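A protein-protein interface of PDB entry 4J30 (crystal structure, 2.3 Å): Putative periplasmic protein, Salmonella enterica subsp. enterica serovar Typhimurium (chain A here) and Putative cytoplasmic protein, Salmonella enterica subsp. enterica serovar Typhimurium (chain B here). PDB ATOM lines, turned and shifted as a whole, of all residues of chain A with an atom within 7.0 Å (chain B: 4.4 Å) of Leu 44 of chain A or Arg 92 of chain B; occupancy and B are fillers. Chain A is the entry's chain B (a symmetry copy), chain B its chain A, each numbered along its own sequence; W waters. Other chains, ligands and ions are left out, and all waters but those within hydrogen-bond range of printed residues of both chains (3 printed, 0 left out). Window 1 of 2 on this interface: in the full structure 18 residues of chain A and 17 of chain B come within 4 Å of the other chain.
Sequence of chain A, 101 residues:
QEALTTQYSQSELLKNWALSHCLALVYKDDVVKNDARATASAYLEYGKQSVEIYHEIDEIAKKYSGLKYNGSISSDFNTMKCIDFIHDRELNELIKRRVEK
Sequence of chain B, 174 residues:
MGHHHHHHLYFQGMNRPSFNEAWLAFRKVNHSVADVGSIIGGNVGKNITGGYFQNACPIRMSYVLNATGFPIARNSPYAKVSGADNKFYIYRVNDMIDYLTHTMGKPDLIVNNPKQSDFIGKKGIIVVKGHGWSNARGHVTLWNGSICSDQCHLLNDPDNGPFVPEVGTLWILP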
ATOM      1  N   THR A   5     -23.437  29.434   8.107  1.00  0.00           N
ATOM      2  CA  THR A   5     -23.921  29.289   9.482  1.00  0.00           C
ATOM      3  C   THR A   5     -25.306  29.895   9.774  1.00  0.00           C
ATOM      4  O   THR A   5     -26.112  29.275  10.468  1.00  0.00           O
ATOM      5  CB  THR A   5     -22.886  29.853  10.487  1.00  0.00           C
ATOM      6  OG1 THR A   5     -21.565  29.633   9.977  1.00  0.00           O
ATOM      7  CG2 THR A   5     -23.019  29.166  11.857  1.00  0.00           C
ATOM      8  N   GLN A  10     -32.876  25.517  13.239  1.00  0.00           N
ATOM      9  CA  GLN A  10     -32.482  25.232  14.610  1.00  0.00           C
ATOM     10  C   GLN A  10     -32.050  23.778  14.808  1.00  0.00           C
ATOM     11  O   GLN A  10     -31.048  23.507  15.475  1.00  0.00           O
ATOM     12  CB  GLN A  10     -33.600  25.632  15.598  1.00  0.00           C
ATOM     13  CG  GLN A  10     -33.760  27.137  15.797  1.00  0.00           C
ATOM     14  CD  GLN A  10     -32.594  27.746  16.560  1.00  0.00           C
ATOM     15  OE1 GLN A  10     -32.347  27.390  17.717  1.00  0.00           O
ATOM     16  NE2 GLN A  10     -31.869  28.682  15.916  1.00  0.00           N
ATOM     17  N   LEU A  13     -28.752  23.258  12.953  1.00  0.00           N
ATOM     18  CA  LEU A  13     -27.661  23.741  13.812  1.00  0.00           C
ATOM     19  C   LEU A  13     -27.299  22.715  14.895  1.00  0.00           C
ATOM     20  O   LEU A  13     -26.121  22.485  15.176  1.00  0.00           O
ATOM     21  CB  LEU A  13     -28.026  25.078  14.470  1.00  0.00           C
ATOM     22  CG  LEU A  13     -28.134  26.356  13.629  1.00  0.00           C
ATOM     23  CD1 LEU A  13     -28.770  27.497  14.458  1.00  0.00           C
ATOM     24  CD2 LEU A  13     -26.760  26.763  13.112  1.00  0.00           C
ATOM     25  N   LEU A  14     -28.305  22.086  15.490  1.00  0.00           N
ATOM     26  CA  LEU A  14     -28.050  21.091  16.544  1.00  0.00           C
ATOM     27  C   LEU A  14     -27.371  19.832  15.996  1.00  0.00           C
ATOM     28  O   LEU A  14     -26.483  19.262  16.641  1.00  0.00           O
ATOM     29  CB  LEU A  14     -29.320  20.762  17.318  1.00  0.00           C
ATOM     30  CG  LEU A  14     -29.866  21.847  18.274  1.00  0.00           C
ATOM     31  CD1 LEU A  14     -31.298  21.536  18.689  1.00  0.00           C
ATOM     32  CD2 LEU A  14     -28.992  22.022  19.513  1.00  0.00           C
ATOM     33  N   TRP A  17     -23.832  20.896  15.206  1.00  0.00           N
ATOM     34  CA  TRP A  17     -23.119  20.921  16.481  1.00  0.00           C
ATOM     35  C   TRP A  17     -22.698  19.510  16.904  1.00  0.00           C
ATOM     36  O   TRP A  17     -21.540  19.275  17.282  1.00  0.00           O
ATOM     37  CB  TRP A  17     -23.971  21.554  17.585  1.00  0.00           C
ATOM     38  CG  TRP A  17     -23.138  21.861  18.805  1.00  0.00           C
ATOM     39  CD1 TRP A  17     -22.501  23.029  19.078  1.00  0.00           C
ATOM     40  CD2 TRP A  17     -22.817  20.961  19.879  1.00  0.00           C
ATOM     41  NE1 TRP A  17     -21.815  22.928  20.270  1.00  0.00           N
ATOM     42  CE2 TRP A  17     -21.983  21.665  20.775  1.00  0.00           C
ATOM     43  CE3 TRP A  17     -23.165  19.630  20.181  1.00  0.00           C
ATOM     44  CZ2 TRP A  17     -21.486  21.083  21.960  1.00  0.00           C
ATOM     45  CZ3 TRP A  17     -22.669  19.058  21.344  1.00  0.00           C
ATOM     46  CH2 TRP A  17     -21.846  19.785  22.223  1.00  0.00           C
ATOM     47  N   THR A  39     -15.636  25.333  15.476  1.00  0.00           N
ATOM     48  CA  THR A  39     -16.744  25.107  14.565  1.00  0.00           C
ATOM     49  C   THR A  39     -18.055  24.802  15.311  1.00  0.00           C
ATOM     50  O   THR A  39     -19.096  25.387  14.995  1.00  0.00           O
ATOM     51  CB  THR A  39     -16.407  23.966  13.570  1.00  0.00           C
ATOM     52  OG1 THR A  39     -15.271  24.342  12.775  1.00  0.00           O
ATOM     53  CG2 THR A  39     -17.593  23.649  12.666  1.00  0.00           C
ATOM     54  N   ALA A  40     -18.008  23.882  16.276  1.00  0.00           N
ATOM     55  CA  ALA A  40     -19.160  23.608  17.129  1.00  0.00           C
ATOM     56  C   ALA A  40     -19.694  24.880  17.826  1.00  0.00           C
ATOM     57  O   ALA A  40     -20.907  25.111  17.837  1.00  0.00           O
ATOM     58  CB  ALA A  40     -18.824  22.503  18.185  1.00  0.00           C
ATOM     59  N   SER A  41     -18.795  25.714  18.368  1.00  0.00           N
ATOM     60  CA  SER A  41     -19.219  26.936  19.073  1.00  0.00           C
ATOM     61  C   SER A  41     -20.014  27.891  18.176  1.00  0.00           C
ATOM     62  O   SER A  41     -20.939  28.578  18.648  1.00  0.00           O
ATOM     63  CB  SER A  41     -18.028  27.651  19.738  1.00  0.00           C
ATOM     64  OG  SER A  41     -17.284  28.425  18.813  1.00  0.00           O
ATOM     65  N   ALA A  42     -19.661  27.935  16.889  1.00  0.00           N
ATOM     66  CA  ALA A  42     -20.418  28.717  15.922  1.00  0.00           C
ATOM     67  C   ALA A  42     -21.898  28.286  15.846  1.00  0.00           C
ATOM     68  O   ALA A  42     -22.783  29.130  15.794  1.00  0.00           O
ATOM     69  CB  ALA A  42     -19.772  28.628  14.547  1.00  0.00           C
ATOM     70  N   TYR A  43     -22.153  26.976  15.825  1.00  0.00           N
ATOM     71  CA  TYR A  43     -23.527  26.442  15.826  1.00  0.00           C
ATOM     72  C   TYR A  43     -24.245  26.683  17.158  1.00  0.00           C
ATOM     73  O   TYR A  43     -25.462  26.924  17.181  1.00  0.00           O
ATOM     74  CB  TYR A  43     -23.547  24.951  15.424  1.00  0.00           C
ATOM     75  CG  TYR A  43     -22.892  24.742  14.073  1.00  0.00           C
ATOM     76  CD1 TYR A  43     -23.317  25.484  12.959  1.00  0.00           C
ATOM     77  CD2 TYR A  43     -21.837  23.846  13.909  1.00  0.00           C
ATOM     78  CE1 TYR A  43     -22.709  25.341  11.710  1.00  0.00           C
ATOM     79  CE2 TYR A  43     -21.211  23.692  12.635  1.00  0.00           C
ATOM     80  CZ  TYR A  43     -21.663  24.442  11.554  1.00  0.00           C
ATOM     81  OH  TYR A  43     -21.083  24.329  10.312  1.00  0.00           O
ATOM     82  N   LEU A  44     -23.495  26.638  18.261  1.00  0.00           N
ATOM     83  CA  LEU A  44     -24.047  27.007  19.559  1.00  0.00           C
ATOM     84  C   LEU A  44     -24.472  28.481  19.575  1.00  0.00           C
ATOM     85  O   LEU A  44     -25.519  28.801  20.102  1.00  0.00           O
ATOM     86  CB  LEU A  44     -23.085  26.668  20.717  1.00  0.00           C
ATOM     87  CG  LEU A  44     -23.542  26.909  22.174  1.00  0.00           C
ATOM     88  CD1 LEU A  44     -22.928  25.889  23.117  1.00  0.00           C
ATOM     89  CD2 LEU A  44     -23.190  28.314  22.639  1.00  0.00           C
ATOM     90  N   GLU A  45     -23.679  29.365  18.974  1.00  0.00           N
ATOM     91  CA  GLU A  45     -23.995  30.792  18.944  1.00  0.00           C
ATOM     92  C   GLU A  45     -25.412  31.057  18.431  1.00  0.00           C
ATOM     93  O   GLU A  45     -26.135  31.893  18.985  1.00  0.00           O
ATOM     94  CB  GLU A  45     -22.971  31.575  18.102  1.00  0.00           C
ATOM     95  CG  GLU A  45     -23.422  33.011  17.678  1.00  0.00           C
ATOM     96  CD  GLU A  45     -23.537  34.003  18.847  1.00  0.00           C
ATOM     97  OE1 GLU A  45     -22.800  33.871  19.846  1.00  0.00           O
ATOM     98  OE2 GLU A  45     -24.350  34.943  18.764  1.00  0.00           O
ATOM     99  N   TYR A  46     -25.798  30.348  17.373  1.00  0.00           N
ATOM    100  CA  TYR A  46     -27.032  30.630  16.666  1.00  0.00           C
ATOM    101  C   TYR A  46     -28.216  29.837  17.187  1.00  0.00           C
ATOM    102  O   TYR A  46     -29.364  30.100  16.796  1.00  0.00           O
ATOM    103  CB  TYR A  46     -26.848  30.416  15.156  1.00  0.00           C
ATOM    104  CG  TYR A  46     -25.986  31.475  14.521  1.00  0.00           C
ATOM    105  CD1 TYR A  46     -26.501  32.740  14.248  1.00  0.00           C
ATOM    106  CD2 TYR A  46     -24.648  31.231  14.232  1.00  0.00           C
ATOM    107  CE1 TYR A  46     -25.710  33.734  13.686  1.00  0.00           C
ATOM    108  CE2 TYR A  46     -23.848  32.211  13.664  1.00  0.00           C
ATOM    109  CZ  TYR A  46     -24.386  33.463  13.393  1.00  0.00           C
ATOM    110  OH  TYR A  46     -23.619  34.452  12.807  1.00  0.00           O
ATOM    111  N   GLY A  47     -27.938  28.880  18.074  1.00  0.00           N
ATOM    112  CA  GLY A  47     -28.989  28.093  18.729  1.00  0.00           C
ATOM    113  C   GLY A  47     -29.844  28.935  19.651  1.00  0.00           C
ATOM    114  O   GLY A  47     -29.418  30.005  20.102  1.00  0.00           O
ATOM    115  N   LYS A  48     -31.056  28.451  19.919  1.00  0.00           N
ATOM    116  CA  LYS A  48     -31.983  29.097  20.839  1.00  0.00           C
ATOM    117  C   LYS A  48     -32.180  28.242  22.083  1.00  0.00           C
ATOM    118  O   LYS A  48     -33.018  28.550  22.944  1.00  0.00           O
ATOM    119  CB  LYS A  48     -33.333  29.370  20.150  1.00  0.00           C
ATOM    120  CG  LYS A  48     -33.270  30.470  19.066  1.00  0.00           C
ATOM    121  CD  LYS A  48     -32.927  31.836  19.674  1.00  0.00           C
ATOM    122  CE  LYS A  48     -32.706  32.915  18.593  1.00  0.00           C
ATOM    123  NZ  LYS A  48     -32.519  34.268  19.220  1.00  0.00           N
ATOM    124  N   GLN A  49     -31.388  27.174  22.169  1.00  0.00           N
ATOM    125  CA  GLN A  49     -31.525  26.181  23.225  1.00  0.00           C
ATOM    126  C   GLN A  49     -30.559  26.438  24.364  1.00  0.00           C
ATOM    127  O   GLN A  49     -29.476  26.987  24.161  1.00  0.00           O
ATOM    128  CB  GLN A  49     -31.306  24.753  22.673  1.00  0.00           C
ATOM    129  CG  GLN A  49     -32.302  24.310  21.603  1.00  0.00           C
ATOM    130  CD  GLN A  49     -32.104  25.058  20.294  1.00  0.00           C
ATOM    131  OE1 GLN A  49     -30.969  25.277  19.868  1.00  0.00           O
ATOM    132  NE2 GLN A  49     -33.207  25.462  19.658  1.00  0.00           N
ATOM    133  N   SER A  50     -30.969  26.024  25.556  1.00  0.00           N
ATOM    134  CA  SER A  50     -30.150  26.062  26.755  1.00  0.00           C
ATOM    135  C   SER A  50     -28.957  25.115  26.624  1.00  0.00           C
ATOM    136  O   SER A  50     -29.001  24.172  25.836  1.00  0.00           O
ATOM    137  CB  SER A  50     -31.008  25.664  27.956  1.00  0.00           C
ATOM    138  OG  SER A  50     -32.013  26.643  28.176  1.00  0.00           O
ATOM    139  N   VAL A  51     -27.912  25.358  27.416  1.00  0.00           N
ATOM    140  CA  VAL A  51     -26.656  24.610  27.300  1.00  0.00           C
ATOM    141  C   VAL A  51     -26.819  23.111  27.577  1.00  0.00           C
ATOM    142  O   VAL A  51     -26.109  22.300  27.004  1.00  0.00           O
ATOM    143  CB  VAL A  51     -25.512  25.244  28.170  1.00  0.00           C
ATOM    144  CG1 VAL A  51     -25.629  24.856  29.665  1.00  0.00           C
ATOM    145  CG2 VAL A  51     -24.143  24.885  27.605  1.00  0.00           C
ATOM    146  N   ILE A  53     -28.887  21.008  26.461  1.00  0.00           N
ATOM    147  CA  ILE A  53     -29.174  20.142  25.304  1.00  0.00           C
ATOM    148  C   ILE A  53     -27.881  19.666  24.640  1.00  0.00           C
ATOM    149  O   ILE A  53     -27.792  18.530  24.183  1.00  0.00           O
ATOM    150  CB  ILE A  53     -30.204  20.708  24.277  1.00  0.00           C
ATOM    151  CG1 ILE A  53     -30.838  19.540  23.494  1.00  0.00           C
ATOM    152  CG2 ILE A  53     -29.565  21.739  23.318  1.00  0.00           C
ATOM    153  CD1 ILE A  53     -31.940  19.947  22.506  1.00  0.00           C
ATOM    154  N   TYR A  54     -26.883  20.549  24.621  1.00  0.00           N
ATOM    155  CA  TYR A  54     -25.548  20.238  24.134  1.00  0.00           C
ATOM    156  C   TYR A  54     -24.833  19.240  25.049  1.00  0.00           C
ATOM    157  O   TYR A  54     -24.174  18.321  24.555  1.00  0.00           O
ATOM    158  CB  TYR A  54     -24.729  21.534  23.978  1.00  0.00           C
ATOM    159  CG  TYR A  54     -25.417  22.571  23.111  1.00  0.00           C
ATOM    160  CD1 TYR A  54     -25.327  22.515  21.709  1.00  0.00           C
ATOM    161  CD2 TYR A  54     -26.169  23.591  23.680  1.00  0.00           C
ATOM    162  CE1 TYR A  54     -25.954  23.459  20.899  1.00  0.00           C
ATOM    163  CE2 TYR A  54     -26.817  24.558  22.872  1.00  0.00           C
ATOM    164  CZ  TYR A  54     -26.704  24.478  21.490  1.00  0.00           C
ATOM    165  OH  TYR A  54     -27.328  25.416  20.700  1.00  0.00           O
ATOM    166  N   TYR B  52     -17.368  23.742  25.393  1.00  0.00           N
ATOM    167  CA  TYR B  52     -18.685  24.134  24.887  1.00  0.00           C
ATOM    168  C   TYR B  52     -18.685  25.607  24.525  1.00  0.00           C
ATOM    169  O   TYR B  52     -19.344  26.013  23.568  1.00  0.00           O
ATOM    170  CB  TYR B  52     -19.777  23.862  25.927  1.00  0.00           C
ATOM    171  CG  TYR B  52     -19.976  22.399  26.238  1.00  0.00           C
ATOM    172  CD1 TYR B  52     -20.864  21.643  25.499  1.00  0.00           C
ATOM    173  CD2 TYR B  52     -19.273  21.774  27.275  1.00  0.00           C
ATOM    174  CE1 TYR B  52     -21.060  20.290  25.757  1.00  0.00           C
ATOM    175  CE2 TYR B  52     -19.460  20.409  27.553  1.00  0.00           C
ATOM    176  CZ  TYR B  52     -20.366  19.687  26.776  1.00  0.00           C
ATOM    177  OH  TYR B  52     -20.605  18.361  27.008  1.00  0.00           O
ATOM    178  N   PRO B  58     -18.956  37.432  24.991  1.00  0.00           N
ATOM    179  CA  PRO B  58     -20.099  37.783  25.842  1.00  0.00           C
ATOM    180  C   PRO B  58     -19.885  37.425  27.311  1.00  0.00           C
ATOM    181  O   PRO B  58     -20.515  38.011  28.211  1.00  0.00           O
ATOM    182  CB  PRO B  58     -21.253  36.985  25.232  1.00  0.00           C
ATOM    183  CG  PRO B  58     -20.610  35.814  24.572  1.00  0.00           C
ATOM    184  CD  PRO B  58     -19.237  36.250  24.146  1.00  0.00           C
ATOM    185  N   ALA B  79     -30.028  32.967  27.581  1.00  0.00           N
ATOM    186  CA  ALA B  79     -29.242  31.826  28.035  1.00  0.00           C
ATOM    187  C   ALA B  79     -27.990  32.279  28.798  1.00  0.00           C
ATOM    188  O   ALA B  79     -27.221  33.134  28.324  1.00  0.00           O
ATOM    189  CB  ALA B  79     -28.873  30.939  26.855  1.00  0.00           C
ATOM    190  N   ILE B  90     -23.829  35.490  30.359  1.00  0.00           N
ATOM    191  CA  ILE B  90     -24.438  35.252  29.062  1.00  0.00           C
ATOM    192  C   ILE B  90     -23.339  34.767  28.121  1.00  0.00           C
ATOM    193  O   ILE B  90     -22.226  35.286  28.135  1.00  0.00           O
ATOM    194  CB  ILE B  90     -25.127  36.547  28.535  1.00  0.00           C
ATOM    195  CG1 ILE B  90     -26.442  36.804  29.292  1.00  0.00           C
ATOM    196  CG2 ILE B  90     -25.346  36.512  26.993  1.00  0.00           C
ATOM    197  CD1 ILE B  90     -27.016  38.238  29.082  1.00  0.00           C
ATOM    198  N   TYR B  91     -23.646  33.769  27.303  1.00  0.00           N
ATOM    199  CA  TYR B  91     -22.607  33.146  26.495  1.00  0.00           C
ATOM    200  C   TYR B  91     -22.787  33.242  24.978  1.00  0.00           C
ATOM    201  O   TYR B  91     -21.925  32.787  24.229  1.00  0.00           O
ATOM    202  CB  TYR B  91     -22.385  31.702  26.942  1.00  0.00           C
ATOM    203  CG  TYR B  91     -23.607  30.807  26.880  1.00  0.00           C
ATOM    204  CD1 TYR B  91     -23.958  30.166  25.692  1.00  0.00           C
ATOM    205  CD2 TYR B  91     -24.390  30.575  28.012  1.00  0.00           C
ATOM    206  CE1 TYR B  91     -25.059  29.331  25.620  1.00  0.00           C
ATOM    207  CE2 TYR B  91     -25.497  29.726  27.951  1.00  0.00           C
ATOM    208  CZ  TYR B  91     -25.815  29.105  26.748  1.00  0.00           C
ATOM    209  OH  TYR B  91     -26.900  28.271  26.642  1.00  0.00           O
ATOM    210  N   ARG B  92     -23.894  33.839  24.538  1.00  0.00           N
ATOM    211  CA  ARG B  92     -24.101  34.173  23.129  1.00  0.00           C
ATOM    212  C   ARG B  92     -23.961  35.677  22.888  1.00  0.00           C
ATOM    213  O   ARG B  92     -24.492  36.496  23.647  1.00  0.00           O
ATOM    214  CB  ARG B  92     -25.467  33.667  22.628  1.00  0.00           C
ATOM    215  CG  ARG B  92     -25.653  32.154  22.763  1.00  0.00           C
ATOM    216  CD  ARG B  92     -26.984  31.691  22.201  1.00  0.00           C
ATOM    217  NE  ARG B  92     -26.958  30.247  21.980  1.00  0.00           N
ATOM    218  CZ  ARG B  92     -27.718  29.363  22.612  1.00  0.00           C
ATOM    219  NH1 ARG B  92     -28.629  29.769  23.494  1.00  0.00           N
ATOM    220  NH2 ARG B  92     -27.587  28.072  22.333  1.00  0.00           N
ATOM    221  N   VAL B  93     -23.233  36.025  21.831  1.00  0.00           N
ATOM    222  CA  VAL B  93     -23.014  37.410  21.435  1.00  0.00           C
ATOM    223  C   VAL B  93     -24.329  38.143  21.135  1.00  0.00           C
ATOM    224  O   VAL B  93     -24.540  39.280  21.594  1.00  0.00           O
ATOM    225  CB  VAL B  93     -22.057  37.491  20.212  1.00  0.00           C
ATOM    226  CG1 VAL B  93     -21.932  38.939  19.675  1.00  0.00           C
ATOM    227  CG2 VAL B  93     -20.689  36.912  20.572  1.00  0.00           C
ATOM    228  N   ASN B  94     -25.217  37.499  20.380  1.00  0.00           N
ATOM    229  CA  ASN B  94     -26.511  38.079  20.023  1.00  0.00           C
ATOM    230  C   ASN B  94     -27.365  38.366  21.257  1.00  0.00           C
ATOM    231  O   ASN B  94     -28.084  39.365  21.318  1.00  0.00           O
ATOM    232  CB  ASN B  94     -27.275  37.157  19.058  1.00  0.00           C
ATOM    233  CG  ASN B  94     -26.982  37.452  17.586  1.00  0.00           C
ATOM    234  OD1 ASN B  94     -26.380  38.478  17.240  1.00  0.00           O
ATOM    235  ND2 ASN B  94     -27.416  36.542  16.706  1.00  0.00           N
ATOM    236  N   ASP B  95     -27.290  37.458  22.232  1.00  0.00           N
ATOM    237  CA  ASP B  95     -27.998  37.611  23.503  1.00  0.00           C
ATOM    238  C   ASP B  95     -27.422  38.785  24.296  1.00  0.00           C
ATOM    239  O   ASP B  95     -28.160  39.566  24.879  1.00  0.00           O
ATOM    240  CB  ASP B  95     -27.893  36.339  24.361  1.00  0.00           C
ATOM    241  CG  ASP B  95     -28.900  35.269  23.978  1.00  0.00           C
ATOM    242  OD1 ASP B  95     -29.770  35.507  23.118  1.00  0.00           O
ATOM    243  OD2 ASP B  95     -28.816  34.163  24.542  1.00  0.00           O
ATOM    244  N   MET B  96     -26.099  38.890  24.315  1.00  0.00           N
ATOM    245  CA  MET B  96     -25.409  39.951  25.037  1.00  0.00           C
ATOM    246  C   MET B  96     -25.790  41.312  24.447  1.00  0.00           C
ATOM    247  O   MET B  96     -26.105  42.253  25.179  1.00  0.00           O
ATOM    248  CB  MET B  96     -23.895  39.724  24.989  1.00  0.00           C
ATOM    249  CG  MET B  96     -23.055  40.587  25.929  1.00  0.00           C
ATOM    250  SD  MET B  96     -23.371  40.308  27.868  1.00  0.00           S
ATOM    251  CE  MET B  96     -24.588  41.802  28.046  1.00  0.00           C
HETATM  252  O   HOH W   1     -19.854  24.615  21.294  1.00  0.00           O
HETATM  253  O   HOH W   2     -24.079  36.580  16.608  1.00  0.00           O
HETATM  254  O   HOH W   3     -28.270  27.828  29.105  1.00  0.00           O
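Hydrophobic or aromatic side chains of chain B within 4 Å of the printed part of chain A: Tyr 52, Tyr 91 and Val 93.
Printed residues of chain A that touch a printed residue of chain B: Trp 17, Leu 44, Glu 45, Gly 47, Gln 49, Ser 50, Val 51 and Tyr 54.
Among the printed residues, 14 pairs touch across the chains.
The side-chain amide oxygen of Gln 10 of chain A sits at hydrogen-bond distance from the side-chain amide nitrogen of Gln 49 of chain A, at 2.9 Å.
NE1 of Trp 17 of chain A lies close to O of Ala 40 of chain A (3.4 Å).
Among the printed residues, pairs that only touch across the chains: Trp 17 of chain A with Tyr 52 of chain B, Leu 44 of chain A with Tyr 52 of chain B, Leu 44 of chain A with Tyr 91 of chain B, Glu 45 of chain A with Arg 92 of chain B, Gln 49 of chain A with Tyr 91 of chain B, Ser 50 of chain A with Tyr 91 of chain B and Tyr 54 of chain A with Tyr 52 of chain B.
The backbone NH (N) of Val 93 of chain B sits at hydrogen-bond distance from the side-chain carboxylate (OE1) of Glu 45 of chain A (3.0 Å).
N of Val 51 of chain A sits at hydrogen-bond distance from OH of Tyr 91 of chain B (3.2 Å).
N of Asn 94 of chain B lies within hydrogen-bond range of OE2 of Glu 45 of chain A (3.1 Å).
The guanidinium group (NE) of Arg 92 of chain B is in hydrogen-bond range of the backbone carbonyl oxygen (O) of Leu 44 of chain A (2.8 Å).
O of Gly 47 of chain A sits close to NE of Arg 92 of chain B (3.1 Å).
The side-chain hydroxyl (OH) of Tyr 54 of chain A lies within hydrogen-bond range of the guanidinium group (NH2) of Arg 92 of chain B.
The backbone carbonyl oxygen of Gln 49 of chain A sits at hydrogen-bond distance from the guanidinium group of Arg 92 of chain B.
Water W1 lies within hydrogen-bond range of the backbone carbonyl oxygen (O) of Tyr 52 of chain B (2.7 Å), the indole nitrogen (NE1) of Trp 17 of chain A (2.8 Å) and the backbone NH (N) of Ser 41 of chain A (3.3 Å).
Water W2 lies within hydrogen-bond range of the side-chain carboxylate (OE2) of Glu 45 of chain A (2.7 Å) and the side-chain amide oxygen (OD1) of Asn 94 of chain B (3.0 Å).
Water W3 bridges OH of Tyr 91 of chain B and N of Val 51 of chain A.
Ala 40 of chain A touches none of the printed residues of chain B.
Tyr 43 of chain A touches none of the printed residues of chain B.
Of chain B, only Tyr 52, Tyr 91 and Arg 92 come within 4 Å of Leu 44 of chain A.
Printed residues of chain B within 4 Å of Ser 50 of chain A: Tyr 91.
Printed residues of chain B within 4 Å of Tyr 54 of chain A: Tyr 52 and Arg 92.
Arg 92 of chain B touches just these residues of chain A: Leu 44 (2.8 Å), Glu 45 (3.3 Å), Gly 47 (3.1 Å), Gln 49 (2.8 Å) and Tyr 54 (3.1 Å).
Of the printed residues of chain A, Val 93 of chain B touches Glu 45.
The nearest printed residue of chain B that does not touch Leu 44 of chain A is Ala 79 of chain B (7.5 Å).
The nearest residue of chain A that does not touch Arg 92 of chain B is Lys 48 of chain A (4.1 Å).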
